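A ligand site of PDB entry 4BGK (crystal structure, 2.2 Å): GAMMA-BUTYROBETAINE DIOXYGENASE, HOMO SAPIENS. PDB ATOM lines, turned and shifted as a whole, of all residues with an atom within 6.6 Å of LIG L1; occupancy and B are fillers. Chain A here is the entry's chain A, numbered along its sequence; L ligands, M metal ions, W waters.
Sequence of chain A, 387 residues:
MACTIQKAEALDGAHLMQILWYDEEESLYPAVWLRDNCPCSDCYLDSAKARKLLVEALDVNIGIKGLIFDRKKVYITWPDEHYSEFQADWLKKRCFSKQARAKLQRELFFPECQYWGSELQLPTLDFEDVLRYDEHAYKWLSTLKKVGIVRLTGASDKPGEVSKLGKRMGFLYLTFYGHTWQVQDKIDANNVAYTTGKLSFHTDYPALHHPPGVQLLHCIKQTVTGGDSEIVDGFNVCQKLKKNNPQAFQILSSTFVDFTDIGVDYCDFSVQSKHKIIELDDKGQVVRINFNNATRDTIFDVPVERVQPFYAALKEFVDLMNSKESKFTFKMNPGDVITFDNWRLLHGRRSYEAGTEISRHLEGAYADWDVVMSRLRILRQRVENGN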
ATOM      1  N   THR A 175     -16.983  27.239  31.124  1.00  0.00           N
ATOM      2  CA  THR A 175     -17.667  26.174  30.388  1.00  0.00           C
ATOM      3  C   THR A 175     -17.071  24.817  30.768  1.00  0.00           C
ATOM      4  O   THR A 175     -16.085  24.737  31.523  1.00  0.00           O
ATOM      5  CB  THR A 175     -17.596  26.353  28.845  1.00  0.00           C
ATOM      6  OG1 THR A 175     -16.273  26.061  28.350  1.00  0.00           O
ATOM      7  CG2 THR A 175     -17.985  27.749  28.433  1.00  0.00           C
ATOM      8  N   TYR A 177     -15.204  23.114  29.128  1.00  0.00           N
ATOM      9  CA  TYR A 177     -13.784  23.028  28.734  1.00  0.00           C
ATOM     10  C   TYR A 177     -12.842  23.778  29.666  1.00  0.00           C
ATOM     11  O   TYR A 177     -11.623  23.748  29.463  1.00  0.00           O
ATOM     12  CB  TYR A 177     -13.601  23.468  27.287  1.00  0.00           C
ATOM     13  CG  TYR A 177     -14.223  22.499  26.329  1.00  0.00           C
ATOM     14  CD1 TYR A 177     -13.583  21.292  26.030  1.00  0.00           C
ATOM     15  CD2 TYR A 177     -15.475  22.741  25.771  1.00  0.00           C
ATOM     16  CE1 TYR A 177     -14.151  20.385  25.162  1.00  0.00           C
ATOM     17  CE2 TYR A 177     -16.055  21.823  24.909  1.00  0.00           C
ATOM     18  CZ  TYR A 177     -15.382  20.639  24.602  1.00  0.00           C
ATOM     19  OH  TYR A 177     -15.932  19.706  23.744  1.00  0.00           O
ATOM     20  N   TRP A 181      -8.553  27.214  28.324  1.00  0.00           N
ATOM     21  CA  TRP A 181      -8.338  25.901  27.692  1.00  0.00           C
ATOM     22  C   TRP A 181      -7.218  25.985  26.681  1.00  0.00           C
ATOM     23  O   TRP A 181      -6.906  27.069  26.155  1.00  0.00           O
ATOM     24  CB  TRP A 181      -9.602  25.359  27.029  1.00  0.00           C
ATOM     25  CG  TRP A 181     -10.589  26.401  26.626  1.00  0.00           C
ATOM     26  CD1 TRP A 181     -11.603  26.874  27.363  1.00  0.00           C
ATOM     27  CD2 TRP A 181     -10.642  27.107  25.376  1.00  0.00           C
ATOM     28  NE1 TRP A 181     -12.283  27.843  26.675  1.00  0.00           N
ATOM     29  CE2 TRP A 181     -11.718  28.007  25.442  1.00  0.00           C
ATOM     30  CE3 TRP A 181      -9.872  27.065  24.206  1.00  0.00           C
ATOM     31  CZ2 TRP A 181     -12.052  28.849  24.411  1.00  0.00           C
ATOM     32  CZ3 TRP A 181     -10.210  27.900  23.187  1.00  0.00           C
ATOM     33  CH2 TRP A 181     -11.286  28.781  23.285  1.00  0.00           C
ATOM     34  N   VAL A 183      -5.550  24.997  23.206  1.00  0.00           N
ATOM     35  CA  VAL A 183      -5.757  24.499  21.853  1.00  0.00           C
ATOM     36  C   VAL A 183      -4.433  23.934  21.371  1.00  0.00           C
ATOM     37  O   VAL A 183      -3.496  24.671  21.068  1.00  0.00           O
ATOM     38  CB  VAL A 183      -6.242  25.590  20.882  1.00  0.00           C
ATOM     39  CG1 VAL A 183      -6.577  24.974  19.533  1.00  0.00           C
ATOM     40  CG2 VAL A 183      -7.428  26.320  21.487  1.00  0.00           C
ATOM     41  N   ASN A 190     -10.891  15.179  22.838  1.00  0.00           N
ATOM     42  CA  ASN A 190     -12.333  15.287  23.114  1.00  0.00           C
ATOM     43  C   ASN A 190     -13.046  16.336  22.226  1.00  0.00           C
ATOM     44  O   ASN A 190     -14.231  16.638  22.404  1.00  0.00           O
ATOM     45  CB  ASN A 190     -12.598  15.563  24.600  1.00  0.00           C
ATOM     46  CG  ASN A 190     -12.142  16.958  25.067  1.00  0.00           C
ATOM     47  OD1 ASN A 190     -11.777  17.821  24.261  1.00  0.00           O
ATOM     48  ND2 ASN A 190     -12.191  17.169  26.364  1.00  0.00           N
ATOM     49  N   ASN A 191     -12.310  16.885  21.266  1.00  0.00           N
ATOM     50  CA  ASN A 191     -12.830  17.975  20.427  1.00  0.00           C
ATOM     51  C   ASN A 191     -11.950  18.095  19.210  1.00  0.00           C
ATOM     52  O   ASN A 191     -10.739  17.941  19.321  1.00  0.00           O
ATOM     53  CB  ASN A 191     -12.852  19.280  21.217  1.00  0.00           C
ATOM     54  CG  ASN A 191     -13.687  20.368  20.550  1.00  0.00           C
ATOM     55  OD1 ASN A 191     -13.234  21.050  19.636  1.00  0.00           O
ATOM     56  ND2 ASN A 191     -14.902  20.571  21.056  1.00  0.00           N
ATOM     57  N   VAL A 192     -12.544  18.324  18.044  1.00  0.00           N
ATOM     58  CA  VAL A 192     -11.783  18.420  16.793  1.00  0.00           C
ATOM     59  C   VAL A 192     -10.741  19.542  16.882  1.00  0.00           C
ATOM     60  O   VAL A 192      -9.671  19.462  16.257  1.00  0.00           O
ATOM     61  CB  VAL A 192     -12.679  18.643  15.545  1.00  0.00           C
ATOM     62  CG1 VAL A 192     -13.567  17.439  15.275  1.00  0.00           C
ATOM     63  CG2 VAL A 192     -13.550  19.886  15.685  1.00  0.00           C
ATOM     64  N   ALA A 193     -11.036  20.573  17.677  1.00  0.00           N
ATOM     65  CA  ALA A 193     -10.108  21.684  17.851  1.00  0.00           C
ATOM     66  C   ALA A 193      -8.770  21.216  18.396  1.00  0.00           C
ATOM     67  O   ALA A 193      -7.725  21.815  18.120  1.00  0.00           O
ATOM     68  CB  ALA A 193     -10.708  22.735  18.766  1.00  0.00           C
ATOM     69  N   TYR A 194      -8.789  20.131  19.158  1.00  0.00           N
ATOM     70  CA  TYR A 194      -7.575  19.638  19.811  1.00  0.00           C
ATOM     71  C   TYR A 194      -6.941  18.516  18.973  1.00  0.00           C
ATOM     72  O   TYR A 194      -6.500  17.498  19.513  1.00  0.00           O
ATOM     73  CB  TYR A 194      -7.889  19.140  21.225  1.00  0.00           C
ATOM     74  CG  TYR A 194      -8.562  20.147  22.163  1.00  0.00           C
ATOM     75  CD1 TYR A 194      -8.336  21.530  22.052  1.00  0.00           C
ATOM     76  CD2 TYR A 194      -9.379  19.707  23.193  1.00  0.00           C
ATOM     77  CE1 TYR A 194      -8.926  22.428  22.920  1.00  0.00           C
ATOM     78  CE2 TYR A 194      -9.988  20.597  24.075  1.00  0.00           C
ATOM     79  CZ  TYR A 194      -9.760  21.951  23.922  1.00  0.00           C
ATOM     80  OH  TYR A 194     -10.363  22.824  24.788  1.00  0.00           O
ATOM     81  N   HIS A 202     -16.787  28.401  11.668  1.00  0.00           N
ATOM     82  CA  HIS A 202     -17.749  28.005  12.673  1.00  0.00           C
ATOM     83  C   HIS A 202     -17.793  29.062  13.729  1.00  0.00           C
ATOM     84  O   HIS A 202     -16.854  29.859  13.871  1.00  0.00           O
ATOM     85  CB  HIS A 202     -17.318  26.665  13.313  1.00  0.00           C
ATOM     86  CG  HIS A 202     -16.060  26.752  14.124  1.00  0.00           C
ATOM     87  ND1 HIS A 202     -14.806  26.763  13.564  1.00  0.00           N
ATOM     88  CD2 HIS A 202     -15.870  26.838  15.456  1.00  0.00           C
ATOM     89  CE1 HIS A 202     -13.899  26.861  14.514  1.00  0.00           C
ATOM     90  NE2 HIS A 202     -14.520  26.899  15.673  1.00  0.00           N
ATOM     91  N   THR A 203     -18.879  29.076  14.482  1.00  0.00           N
ATOM     92  CA  THR A 203     -18.939  29.740  15.777  1.00  0.00           C
ATOM     93  C   THR A 203     -18.644  28.717  16.837  1.00  0.00           C
ATOM     94  O   THR A 203     -18.855  27.527  16.616  1.00  0.00           O
ATOM     95  CB  THR A 203     -20.326  30.377  16.051  1.00  0.00           C
ATOM     96  OG1 THR A 203     -21.369  29.392  16.141  1.00  0.00           O
ATOM     97  CG2 THR A 203     -20.675  31.375  14.955  1.00  0.00           C
ATOM     98  N   ASP A 204     -18.178  29.168  18.002  1.00  0.00           N
ATOM     99  CA  ASP A 204     -17.910  28.272  19.131  1.00  0.00           C
ATOM    100  C   ASP A 204     -19.152  28.024  19.993  1.00  0.00           C
ATOM    101  O   ASP A 204     -19.929  28.946  20.251  1.00  0.00           O
ATOM    102  CB  ASP A 204     -16.770  28.789  20.021  1.00  0.00           C
ATOM    103  CG  ASP A 204     -15.416  28.244  19.596  1.00  0.00           C
ATOM    104  OD1 ASP A 204     -15.260  28.000  18.410  1.00  0.00           O
ATOM    105  OD2 ASP A 204     -14.521  28.060  20.445  1.00  0.00           O
ATOM    106  N   TYR A 205     -19.314  26.761  20.394  1.00  0.00           N
ATOM    107  CA  TYR A 205     -20.304  26.312  21.341  1.00  0.00           C
ATOM    108  C   TYR A 205     -21.787  26.530  20.977  1.00  0.00           C
ATOM    109  O   TYR A 205     -22.571  26.930  21.842  1.00  0.00           O
ATOM    110  CB  TYR A 205     -20.002  26.920  22.707  1.00  0.00           C
ATOM    111  CG  TYR A 205     -19.566  25.928  23.764  1.00  0.00           C
ATOM    112  CD1 TYR A 205     -20.212  24.693  23.926  1.00  0.00           C
ATOM    113  CD2 TYR A 205     -18.528  26.249  24.651  1.00  0.00           C
ATOM    114  CE1 TYR A 205     -19.828  23.822  24.901  1.00  0.00           C
ATOM    115  CE2 TYR A 205     -18.141  25.375  25.642  1.00  0.00           C
ATOM    116  CZ  TYR A 205     -18.795  24.179  25.771  1.00  0.00           C
ATOM    117  OH  TYR A 205     -18.422  23.319  26.773  1.00  0.00           O
ATOM    118  N   PRO A 206     -22.192  26.238  19.727  1.00  0.00           N
ATOM    119  CA  PRO A 206     -23.622  26.216  19.525  1.00  0.00           C
ATOM    120  C   PRO A 206     -24.336  25.075  20.277  1.00  0.00           C
ATOM    121  O   PRO A 206     -25.555  25.141  20.415  1.00  0.00           O
ATOM    122  CB  PRO A 206     -23.774  26.061  18.007  1.00  0.00           C
ATOM    123  CG  PRO A 206     -22.514  25.471  17.562  1.00  0.00           C
ATOM    124  CD  PRO A 206     -21.470  26.044  18.462  1.00  0.00           C
ATOM    125  N   ALA A 207     -23.570  24.098  20.798  1.00  0.00           N
ATOM    126  CA  ALA A 207     -24.138  23.084  21.705  1.00  0.00           C
ATOM    127  C   ALA A 207     -24.730  23.689  22.975  1.00  0.00           C
ATOM    128  O   ALA A 207     -25.465  23.024  23.683  1.00  0.00           O
ATOM    129  CB  ALA A 207     -23.106  22.015  22.059  1.00  0.00           C
ATOM    130  N   GLN A 215     -14.846  35.635  22.382  1.00  0.00           N
ATOM    131  CA  GLN A 215     -13.857  34.598  22.506  1.00  0.00           C
ATOM    132  C   GLN A 215     -12.481  35.261  22.501  1.00  0.00           C
ATOM    133  O   GLN A 215     -12.251  36.210  21.783  1.00  0.00           O
ATOM    134  CB  GLN A 215     -13.992  33.626  21.331  1.00  0.00           C
ATOM    135  CG  GLN A 215     -12.927  32.562  21.299  1.00  0.00           C
ATOM    136  CD  GLN A 215     -13.272  31.417  20.372  1.00  0.00           C
ATOM    137  OE1 GLN A 215     -12.410  30.598  20.069  1.00  0.00           O
ATOM    138  NE2 GLN A 215     -14.521  31.361  19.917  1.00  0.00           N
ATOM    139  N   LEU A 217      -8.307  34.364  22.090  1.00  0.00           N
ATOM    140  CA  LEU A 217      -7.303  33.359  21.698  1.00  0.00           C
ATOM    141  C   LEU A 217      -5.900  33.960  21.695  1.00  0.00           C
ATOM    142  O   LEU A 217      -5.596  34.942  20.999  1.00  0.00           O
ATOM    143  CB  LEU A 217      -7.596  32.788  20.313  1.00  0.00           C
ATOM    144  CG  LEU A 217      -8.721  31.760  20.165  1.00  0.00           C
ATOM    145  CD1 LEU A 217      -8.877  31.372  18.697  1.00  0.00           C
ATOM    146  CD2 LEU A 217      -8.445  30.526  20.990  1.00  0.00           C
ATOM    147  N   ASP A 261     -22.694  17.811  22.348  1.00  0.00           N
ATOM    148  CA  ASP A 261     -21.324  17.660  22.799  1.00  0.00           C
ATOM    149  C   ASP A 261     -21.298  16.747  24.018  1.00  0.00           C
ATOM    150  O   ASP A 261     -21.899  17.066  25.032  1.00  0.00           O
ATOM    151  CB  ASP A 261     -20.684  19.027  23.119  1.00  0.00           C
ATOM    152  CG  ASP A 261     -19.158  18.982  23.142  1.00  0.00           C
ATOM    153  OD1 ASP A 261     -18.533  18.005  22.647  1.00  0.00           O
ATOM    154  OD2 ASP A 261     -18.568  19.945  23.664  1.00  0.00           O
ATOM    155  N   ASP A 265     -14.095  16.844  30.250  1.00  0.00           N
ATOM    156  CA  ASP A 265     -12.988  17.808  30.312  1.00  0.00           C
ATOM    157  C   ASP A 265     -12.974  18.458  31.698  1.00  0.00           C
ATOM    158  O   ASP A 265     -12.493  17.836  32.626  1.00  0.00           O
ATOM    159  CB  ASP A 265     -13.059  18.802  29.163  1.00  0.00           C
ATOM    160  CG  ASP A 265     -11.699  19.457  28.856  1.00  0.00           C
ATOM    161  OD1 ASP A 265     -11.080  20.033  29.758  1.00  0.00           O
ATOM    162  OD2 ASP A 265     -11.274  19.417  27.685  1.00  0.00           O
ATOM    163  N   ASN A 292     -21.602  25.261  14.120  1.00  0.00           N
ATOM    164  CA  ASN A 292     -20.370  24.508  14.104  1.00  0.00           C
ATOM    165  C   ASN A 292     -20.651  23.138  13.490  1.00  0.00           C
ATOM    166  O   ASN A 292     -21.445  22.349  14.019  1.00  0.00           O
ATOM    167  CB  ASN A 292     -19.774  24.420  15.503  1.00  0.00           C
ATOM    168  CG  ASN A 292     -18.413  23.734  15.517  1.00  0.00           C
ATOM    169  OD1 ASN A 292     -18.031  23.063  14.536  1.00  0.00           O
ATOM    170  ND2 ASN A 292     -17.689  23.865  16.626  1.00  0.00           N
ATOM    171  N   ALA A 294     -18.839  20.505  13.301  1.00  0.00           N
ATOM    172  CA  ALA A 294     -18.342  19.369  14.072  1.00  0.00           C
ATOM    173  C   ALA A 294     -19.374  18.880  15.091  1.00  0.00           C
ATOM    174  O   ALA A 294     -19.490  17.670  15.326  1.00  0.00           O
ATOM    175  CB  ALA A 294     -17.025  19.730  14.758  1.00  0.00           C
ATOM    176  N   THR A 295     -20.097  19.819  15.705  1.00  0.00           N
ATOM    177  CA  THR A 295     -20.963  19.541  16.814  1.00  0.00           C
ATOM    178  C   THR A 295     -22.432  19.530  16.431  1.00  0.00           C
ATOM    179  O   THR A 295     -23.279  19.246  17.279  1.00  0.00           O
ATOM    180  CB  THR A 295     -20.780  20.562  17.958  1.00  0.00           C
ATOM    181  OG1 THR A 295     -21.151  21.877  17.535  1.00  0.00           O
ATOM    182  CG2 THR A 295     -19.359  20.590  18.442  1.00  0.00           C
ATOM    183  N   TYR A 366     -13.601  32.411  27.113  1.00  0.00           N
ATOM    184  CA  TYR A 366     -14.807  33.035  26.648  1.00  0.00           C
ATOM    185  C   TYR A 366     -15.216  34.151  27.616  1.00  0.00           C
ATOM    186  O   TYR A 366     -14.883  34.103  28.803  1.00  0.00           O
ATOM    187  CB  TYR A 366     -15.923  32.004  26.588  1.00  0.00           C
ATOM    188  CG  TYR A 366     -15.706  30.878  25.589  1.00  0.00           C
ATOM    189  CD1 TYR A 366     -15.504  31.159  24.224  1.00  0.00           C
ATOM    190  CD2 TYR A 366     -15.697  29.558  26.002  1.00  0.00           C
ATOM    191  CE1 TYR A 366     -15.323  30.132  23.309  1.00  0.00           C
ATOM    192  CE2 TYR A 366     -15.507  28.541  25.104  1.00  0.00           C
ATOM    193  CZ  TYR A 366     -15.344  28.825  23.759  1.00  0.00           C
ATOM    194  OH  TYR A 366     -15.148  27.787  22.886  1.00  0.00           O
HETATM  195  O1  LIG L   1     -18.203  24.493  19.345  1.00  0.00           O
HETATM  196  P1  LIG L   1     -16.940  24.031  20.000  1.00  0.00           P
HETATM  197  O2  LIG L   1     -16.900  22.521  20.183  1.00  0.00           O
HETATM  198  C1  LIG L   1     -16.774  24.923  21.572  1.00  0.00           C
HETATM  199  C2  LIG L   1     -15.595  24.412  22.389  1.00  0.00           C
HETATM  200  C3  LIG L   1     -14.285  24.809  21.731  1.00  0.00           C
HETATM  201  N1  LIG L   1     -13.060  24.516  22.524  1.00  0.00           N
HETATM  202  C4  LIG L   1     -12.841  23.064  22.725  1.00  0.00           C
HETATM  203  C5  LIG L   1     -13.061  25.196  23.834  1.00  0.00           C
HETATM  204  C6  LIG L   1     -11.946  25.042  21.704  1.00  0.00           C
HETATM  205  C1  LG2 L   2     -11.238  26.690  18.480  1.00  0.00           C
HETATM  206  C2  LG2 L   2     -10.634  27.370  17.317  1.00  0.00           C
HETATM  207  C3  LG2 L   2      -8.689  28.290  16.184  1.00  0.00           C
HETATM  208  C4  LG2 L   2      -7.248  27.868  15.973  1.00  0.00           C
HETATM  209  O1  LG2 L   2     -10.496  26.084  19.308  1.00  0.00           O
HETATM  210  O2  LG2 L   2     -12.492  26.751  18.617  1.00  0.00           O
HETATM  211  O3  LG2 L   2     -11.368  27.867  16.492  1.00  0.00           O
HETATM  212  O4  LG2 L   2      -6.575  28.592  15.222  1.00  0.00           O
HETATM  213  N1  LG2 L   2      -9.312  27.470  17.219  1.00  0.00           N
HETATM  214  O5  LG2 L   2      -6.797  26.820  16.516  1.00  0.00           O
HETATM  215 ZN    ZN M   1     -13.452  27.840  17.318  1.00  0.00          ZN
HETATM  216  O   HOH W   1     -15.731  21.577  17.912  1.00  0.00           O
HETATM  217  O   HOH W   2     -18.994  21.923  21.752  1.00  0.00           O
HETATM  218  O   HOH W   3     -20.765  23.256  20.116  1.00  0.00           O
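The side-chain hydroxyl (OH) of Tyr 366 sits at hydrogen-bond distance from the side-chain carboxylate (OD2) of Asp 204. The side-chain hydroxyl of Tyr 177 lies within hydrogen-bond range of the side-chain carboxylate of Asp 261, at 2.6 Å. OD1 of Asn 191 is in hydrogen-bond range of N of Ala 193 (3.0 Å). The side-chain carboxylate of Asp 204 lies close to the side-chain amide oxygen of Gln 215, at 3.3 Å. ND2 of Asn 191 is in hydrogen-bond range of OH of Tyr 177 (3.0 Å). The side-chain hydroxyl (OG1) of Thr 175 sits close to the backbone NH (N) of Tyr 177 (3.2 Å). The side-chain amide oxygen (OD1) of Asn 292 is in hydrogen-bond range of the backbone NH (N) of Ala 294 (3.0 Å).
Water W2 lies within hydrogen-bond range of O2 of LIG L1 and OD2 of Asp 261. Water W1 lies within hydrogen-bond range of O2 of LIG L1 (2.7 Å), OD1 of Asn 191 (3.1 Å) and ND2 of Asn 292 (3.3 Å). Water W3 lies within hydrogen-bond range of O1 of LIG L1, OG1 of Thr 295 and N of Ala 207.
Residues that only touch LIG L1: Tyr 194, Tyr 366, Trp 181, Asp 204, Thr 295, Tyr 177, Pro 206 and Ala 193. Hydrophobic or aromatic side chains within 4 Å of LIG L1: Tyr 177, Trp 181, Ala 193, Tyr 194, Tyr 205 and Pro 206. Of the 23 residues printed, 11 come within 4 Å of LIG L1.
O1 of LIG L1 lies within hydrogen-bond range of N of Tyr 205, 2.7 Å away. ND2 of Asn 191 is in hydrogen-bond range of O2 of LIG L1 (2.9 Å). O1 of LIG L1 sits at hydrogen-bond distance from ND2 of Asn 292 (2.8 Å).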
